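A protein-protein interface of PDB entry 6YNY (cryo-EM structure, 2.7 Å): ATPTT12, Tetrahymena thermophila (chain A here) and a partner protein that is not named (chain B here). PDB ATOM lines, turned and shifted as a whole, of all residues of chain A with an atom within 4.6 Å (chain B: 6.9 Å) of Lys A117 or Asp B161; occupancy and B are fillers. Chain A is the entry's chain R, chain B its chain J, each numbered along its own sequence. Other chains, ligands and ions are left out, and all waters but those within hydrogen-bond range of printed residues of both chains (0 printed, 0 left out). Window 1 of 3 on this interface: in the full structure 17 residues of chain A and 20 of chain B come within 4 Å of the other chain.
The side-chain carboxylate (OE2) of Glu B165 lies within hydrogen-bond range of the backbone NH (N) of Thr A118 (2.5 Å).
NH2 of Arg B168 lies within hydrogen-bond range of O of Thr A118, at 2.6 Å.
Lys A117 touches Asp B161.
Lys A117 touches Glu B165 (C to OE2, 3.5 Å).
CE of Lys B172 touches CG2 of Thr A118, at 3.7 Å.
Lys A119 touches Arg B168.
The guanidinium group of Arg B168 is in salt-bridge range of the side-chain carboxylate of Glu B165.
Printed residues of chain A that touch a printed residue of chain B: Lys A117, Thr A118 and Lys A119.
Among the printed residues, 6 pairs touch across the chains.
Among the printed residues, no Asp or Glu carboxylate lies within 4 Å of a Lys or Arg side-chain nitrogen of the other chain.
Pro A114 touches none of the printed residues of chain B.
Lys A117 touches just these residues of chain B: Asp B161 and Glu B165.
Of the printed residues of chain B, Lys A119 touches Arg B168.
Pro B156 touches none of the printed residues of chain A.
Asp B161 touches just one residue of chain A: Lys A117.
Of the printed residues of chain A, Glu B165 touches Lys A117 (3.5 Å) and Thr A118 (2.5 Å).
Of the printed residues of chain A, Lys B172 touches Thr A118.
The nearest printed residue of chain A that does not touch Asp B161 is Asp A113 (8.4 Å).
The nearest printed residue of chain A that does not touch Glu B165 is Gln A116 (5.1 Å).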
ATOM      1  N   ASP A 113      32.805  17.532  12.246  1.00  0.00           N
ATOM      2  CA  ASP A 113      32.107  16.260  12.348  1.00  0.00           C
ATOM      3  C   ASP A 113      30.940  16.220  11.366  1.00  0.00           C
ATOM      4  O   ASP A 113      30.021  17.045  11.479  1.00  0.00           O
ATOM      5  CB  ASP A 113      31.611  16.050  13.774  1.00  0.00           C
ATOM      6  CG  ASP A 113      31.047  14.663  13.999  1.00  0.00           C
ATOM      7  OD1 ASP A 113      30.963  13.886  13.026  1.00  0.00           O
ATOM      8  OD2 ASP A 113      30.695  14.347  15.154  1.00  0.00           O
ATOM      9  N   PRO A 114      30.932  15.299  10.400  1.00  0.00           N
ATOM     10  CA  PRO A 114      29.787  15.230   9.480  1.00  0.00           C
ATOM     11  C   PRO A 114      28.494  14.815  10.150  1.00  0.00           C
ATOM     12  O   PRO A 114      27.420  15.241   9.710  1.00  0.00           O
ATOM     13  CB  PRO A 114      30.234  14.194   8.442  1.00  0.00           C
ATOM     14  CG  PRO A 114      31.701  14.139   8.553  1.00  0.00           C
ATOM     15  CD  PRO A 114      32.019  14.404   9.978  1.00  0.00           C
ATOM     16  N   LEU A 115      28.555  13.993  11.196  1.00  0.00           N
ATOM     17  CA  LEU A 115      27.342  13.518  11.843  1.00  0.00           C
ATOM     18  C   LEU A 115      26.587  14.622  12.564  1.00  0.00           C
ATOM     19  O   LEU A 115      25.434  14.408  12.951  1.00  0.00           O
ATOM     20  CB  LEU A 115      27.688  12.404  12.825  1.00  0.00           C
ATOM     21  CG  LEU A 115      28.372  11.192  12.201  1.00  0.00           C
ATOM     22  CD1 LEU A 115      28.737  10.204  13.273  1.00  0.00           C
ATOM     23  CD2 LEU A 115      27.477  10.546  11.168  1.00  0.00           C
ATOM     24  N   GLN A 116      27.202  15.783  12.758  1.00  0.00           N
ATOM     25  CA  GLN A 116      26.528  16.937  13.328  1.00  0.00           C
ATOM     26  C   GLN A 116      25.940  17.847  12.262  1.00  0.00           C
ATOM     27  O   GLN A 116      25.458  18.936  12.587  1.00  0.00           O
ATOM     28  CB  GLN A 116      27.497  17.725  14.209  1.00  0.00           C
ATOM     29  CG  GLN A 116      27.217  17.611  15.691  1.00  0.00           C
ATOM     30  CD  GLN A 116      27.276  16.187  16.192  1.00  0.00           C
ATOM     31  OE1 GLN A 116      28.344  15.580  16.245  1.00  0.00           O
ATOM     32  NE2 GLN A 116      26.121  15.641  16.556  1.00  0.00           N
ATOM     33  N   LYS A 117      25.965  17.424  11.004  1.00  0.00           N
ATOM     34  CA  LYS A 117      25.416  18.188   9.899  1.00  0.00           C
ATOM     35  C   LYS A 117      24.111  17.563   9.426  1.00  0.00           C
ATOM     36  O   LYS A 117      23.791  16.416   9.744  1.00  0.00           O
ATOM     37  CB  LYS A 117      26.415  18.261   8.743  1.00  0.00           C
ATOM     38  CG  LYS A 117      27.694  18.967   9.116  1.00  0.00           C
ATOM     39  CD  LYS A 117      28.613  19.119   7.932  1.00  0.00           C
ATOM     40  CE  LYS A 117      29.862  19.885   8.312  1.00  0.00           C
ATOM     41  NZ  LYS A 117      30.667  20.267   7.126  1.00  0.00           N
ATOM     42  N   THR A 118      23.362  18.340   8.653  1.00  0.00           N
ATOM     43  CA  THR A 118      22.068  17.886   8.167  1.00  0.00           C
ATOM     44  C   THR A 118      22.233  16.660   7.282  1.00  0.00           C
ATOM     45  O   THR A 118      23.076  16.633   6.381  1.00  0.00           O
ATOM     46  CB  THR A 118      21.376  19.008   7.398  1.00  0.00           C
ATOM     47  OG1 THR A 118      21.282  20.171   8.227  1.00  0.00           O
ATOM     48  CG2 THR A 118      19.992  18.583   6.977  1.00  0.00           C
ATOM     49  N   LYS A 119      21.420  15.643   7.543  1.00  0.00           N
ATOM     50  CA  LYS A 119      21.497  14.399   6.797  1.00  0.00           C
ATOM     51  C   LYS A 119      20.708  14.499   5.500  1.00  0.00           C
ATOM     52  O   LYS A 119      19.731  15.245   5.395  1.00  0.00           O
ATOM     53  CB  LYS A 119      20.950  13.239   7.624  1.00  0.00           C
ATOM     54  CG  LYS A 119      21.393  13.213   9.071  1.00  0.00           C
ATOM     55  CD  LYS A 119      22.862  12.912   9.208  1.00  0.00           C
ATOM     56  CE  LYS A 119      23.259  12.825  10.665  1.00  0.00           C
ATOM     57  NZ  LYS A 119      22.551  11.727  11.367  1.00  0.00           N
ATOM     58  N   PRO B 156      38.487  30.612   3.545  1.00  0.00           N
ATOM     59  CA  PRO B 156      39.041  29.304   3.893  1.00  0.00           C
ATOM     60  C   PRO B 156      37.991  28.210   3.790  1.00  0.00           C
ATOM     61  O   PRO B 156      36.786  28.451   3.878  1.00  0.00           O
ATOM     62  CB  PRO B 156      39.531  29.492   5.332  1.00  0.00           C
ATOM     63  CG  PRO B 156      38.836  30.680   5.829  1.00  0.00           C
ATOM     64  CD  PRO B 156      38.595  31.559   4.664  1.00  0.00           C
ATOM     65  N   ASN B 157      38.473  26.984   3.596  1.00  0.00           N
ATOM     66  CA  ASN B 157      37.574  25.871   3.318  1.00  0.00           C
ATOM     67  C   ASN B 157      36.615  25.611   4.469  1.00  0.00           C
ATOM     68  O   ASN B 157      35.464  25.229   4.238  1.00  0.00           O
ATOM     69  CB  ASN B 157      38.382  24.618   2.996  1.00  0.00           C
ATOM     70  CG  ASN B 157      39.037  24.688   1.641  1.00  0.00           C
ATOM     71  OD1 ASN B 157      38.441  25.158   0.674  1.00  0.00           O
ATOM     72  ND2 ASN B 157      40.274  24.229   1.561  1.00  0.00           N
ATOM     73  N   TRP B 158      37.059  25.805   5.711  1.00  0.00           N
ATOM     74  CA  TRP B 158      36.152  25.605   6.832  1.00  0.00           C
ATOM     75  C   TRP B 158      34.965  26.553   6.757  1.00  0.00           C
ATOM     76  O   TRP B 158      33.887  26.239   7.271  1.00  0.00           O
ATOM     77  CB  TRP B 158      36.894  25.774   8.159  1.00  0.00           C
ATOM     78  CG  TRP B 158      37.259  27.176   8.515  1.00  0.00           C
ATOM     79  CD1 TRP B 158      38.477  27.757   8.377  1.00  0.00           C
ATOM     80  CD2 TRP B 158      36.402  28.174   9.083  1.00  0.00           C
ATOM     81  NE1 TRP B 158      38.437  29.053   8.817  1.00  0.00           N
ATOM     82  CE2 TRP B 158      37.171  29.335   9.251  1.00  0.00           C
ATOM     83  CE3 TRP B 158      35.059  28.199   9.456  1.00  0.00           C
ATOM     84  CZ2 TRP B 158      36.645  30.503   9.779  1.00  0.00           C
ATOM     85  CZ3 TRP B 158      34.540  29.360   9.978  1.00  0.00           C
ATOM     86  CH2 TRP B 158      35.329  30.495  10.135  1.00  0.00           C
ATOM     87  N   ALA B 159      35.138  27.709   6.116  1.00  0.00           N
ATOM     88  CA  ALA B 159      34.031  28.640   5.953  1.00  0.00           C
ATOM     89  C   ALA B 159      33.096  28.195   4.837  1.00  0.00           C
ATOM     90  O   ALA B 159      31.874  28.316   4.963  1.00  0.00           O
ATOM     91  CB  ALA B 159      34.564  30.042   5.676  1.00  0.00           C
ATOM     92  N   LEU B 160      33.653  27.678   3.741  1.00  0.00           N
ATOM     93  CA  LEU B 160      32.822  27.177   2.655  1.00  0.00           C
ATOM     94  C   LEU B 160      31.966  26.005   3.106  1.00  0.00           C
ATOM     95  O   LEU B 160      30.836  25.843   2.633  1.00  0.00           O
ATOM     96  CB  LEU B 160      33.698  26.768   1.476  1.00  0.00           C
ATOM     97  CG  LEU B 160      34.627  27.845   0.919  1.00  0.00           C
ATOM     98  CD1 LEU B 160      35.533  27.264  -0.133  1.00  0.00           C
ATOM     99  CD2 LEU B 160      33.843  29.002   0.351  1.00  0.00           C
ATOM    100  N   ASP B 161      32.484  25.177   4.012  1.00  0.00           N
ATOM    101  CA  ASP B 161      31.685  24.090   4.563  1.00  0.00           C
ATOM    102  C   ASP B 161      30.536  24.625   5.407  1.00  0.00           C
ATOM    103  O   ASP B 161      29.415  24.109   5.339  1.00  0.00           O
ATOM    104  CB  ASP B 161      32.573  23.164   5.390  1.00  0.00           C
ATOM    105  CG  ASP B 161      33.562  22.393   4.541  1.00  0.00           C
ATOM    106  OD1 ASP B 161      33.507  22.514   3.300  1.00  0.00           O
ATOM    107  OD2 ASP B 161      34.395  21.663   5.116  1.00  0.00           O
ATOM    108  N   HIS B 162      30.794  25.656   6.212  1.00  0.00           N
ATOM    109  CA  HIS B 162      29.723  26.285   6.975  1.00  0.00           C
ATOM    110  C   HIS B 162      28.660  26.861   6.053  1.00  0.00           C
ATOM    111  O   HIS B 162      27.460  26.651   6.258  1.00  0.00           O
ATOM    112  CB  HIS B 162      30.290  27.377   7.877  1.00  0.00           C
ATOM    113  CG  HIS B 162      30.967  26.859   9.105  1.00  0.00           C
ATOM    114  ND1 HIS B 162      30.952  27.539  10.302  1.00  0.00           N
ATOM    115  CD2 HIS B 162      31.682  25.731   9.323  1.00  0.00           C
ATOM    116  CE1 HIS B 162      31.623  26.850  11.206  1.00  0.00           C
ATOM    117  NE2 HIS B 162      32.077  25.750  10.637  1.00  0.00           N
ATOM    118  N   MET B 163      29.086  27.596   5.026  1.00  0.00           N
ATOM    119  CA  MET B 163      28.136  28.151   4.071  1.00  0.00           C
ATOM    120  C   MET B 163      27.340  27.048   3.389  1.00  0.00           C
ATOM    121  O   MET B 163      26.134  27.187   3.163  1.00  0.00           O
ATOM    122  CB  MET B 163      28.886  28.991   3.042  1.00  0.00           C
ATOM    123  CG  MET B 163      29.651  30.145   3.650  1.00  0.00           C
ATOM    124  SD  MET B 163      30.954  30.802   2.599  1.00  0.00           S
ATOM    125  CE  MET B 163      29.973  31.609   1.351  1.00  0.00           C
ATOM    126  N   LYS B 164      28.001  25.939   3.062  1.00  0.00           N
ATOM    127  CA  LYS B 164      27.311  24.812   2.447  1.00  0.00           C
ATOM    128  C   LYS B 164      26.284  24.207   3.396  1.00  0.00           C
ATOM    129  O   LYS B 164      25.201  23.795   2.967  1.00  0.00           O
ATOM    130  CB  LYS B 164      28.340  23.769   2.016  1.00  0.00           C
ATOM    131  CG  LYS B 164      27.789  22.459   1.513  1.00  0.00           C
ATOM    132  CD  LYS B 164      28.924  21.492   1.264  1.00  0.00           C
ATOM    133  CE  LYS B 164      28.442  20.149   0.753  1.00  0.00           C
ATOM    134  NZ  LYS B 164      27.589  19.430   1.727  1.00  0.00           N
ATOM    135  N   GLU B 165      26.605  24.144   4.688  1.00  0.00           N
ATOM    136  CA  GLU B 165      25.711  23.504   5.647  1.00  0.00           C
ATOM    137  C   GLU B 165      24.584  24.425   6.087  1.00  0.00           C
ATOM    138  O   GLU B 165      23.494  23.946   6.414  1.00  0.00           O
ATOM    139  CB  GLU B 165      26.500  23.025   6.862  1.00  0.00           C
ATOM    140  CG  GLU B 165      25.656  22.347   7.924  1.00  0.00           C
ATOM    141  CD  GLU B 165      24.893  21.150   7.394  1.00  0.00           C
ATOM    142  OE1 GLU B 165      25.287  20.610   6.340  1.00  0.00           O
ATOM    143  OE2 GLU B 165      23.897  20.751   8.030  1.00  0.00           O
ATOM    144  N   LYS B 166      24.823  25.737   6.118  1.00  0.00           N
ATOM    145  CA  LYS B 166      23.749  26.670   6.430  1.00  0.00           C
ATOM    146  C   LYS B 166      22.577  26.493   5.476  1.00  0.00           C
ATOM    147  O   LYS B 166      21.413  26.543   5.888  1.00  0.00           O
ATOM    148  CB  LYS B 166      24.264  28.104   6.372  1.00  0.00           C
ATOM    149  CG  LYS B 166      25.083  28.520   7.566  1.00  0.00           C
ATOM    150  CD  LYS B 166      25.410  29.995   7.525  1.00  0.00           C
ATOM    151  CE  LYS B 166      26.367  30.329   6.407  1.00  0.00           C
ATOM    152  NZ  LYS B 166      26.750  31.757   6.414  1.00  0.00           N
ATOM    153  N   ARG B 168      21.693  23.790   3.886  1.00  0.00           N
ATOM    154  CA  ARG B 168      21.002  22.537   4.146  1.00  0.00           C
ATOM    155  C   ARG B 168      20.160  22.616   5.410  1.00  0.00           C
ATOM    156  O   ARG B 168      19.083  22.012   5.473  1.00  0.00           O
ATOM    157  CB  ARG B 168      22.019  21.406   4.241  1.00  0.00           C
ATOM    158  CG  ARG B 168      22.731  21.141   2.938  1.00  0.00           C
ATOM    159  CD  ARG B 168      23.924  20.240   3.118  1.00  0.00           C
ATOM    160  NE  ARG B 168      23.582  18.975   3.755  1.00  0.00           N
ATOM    161  CZ  ARG B 168      23.033  17.943   3.125  1.00  0.00           C
ATOM    162  NH1 ARG B 168      22.751  18.015   1.832  1.00  0.00           N
ATOM    163  NH2 ARG B 168      22.767  16.834   3.794  1.00  0.00           N
ATOM    164  N   LYS B 172      16.159  22.453   5.687  1.00  0.00           N
ATOM    165  CA  LYS B 172      15.470  21.555   6.604  1.00  0.00           C
ATOM    166  C   LYS B 172      14.426  22.305   7.419  1.00  0.00           C
ATOM    167  O   LYS B 172      13.275  21.867   7.528  1.00  0.00           O
ATOM    168  CB  LYS B 172      16.489  20.883   7.518  1.00  0.00           C
ATOM    169  CG  LYS B 172      15.929  19.799   8.398  1.00  0.00           C
ATOM    170  CD  LYS B 172      16.464  19.904   9.804  1.00  0.00           C
ATOM    171  CE  LYS B 172      17.959  19.765   9.849  1.00  0.00           C
ATOM    172  NZ  LYS B 172      18.468  19.851  11.236  1.00  0.00           N
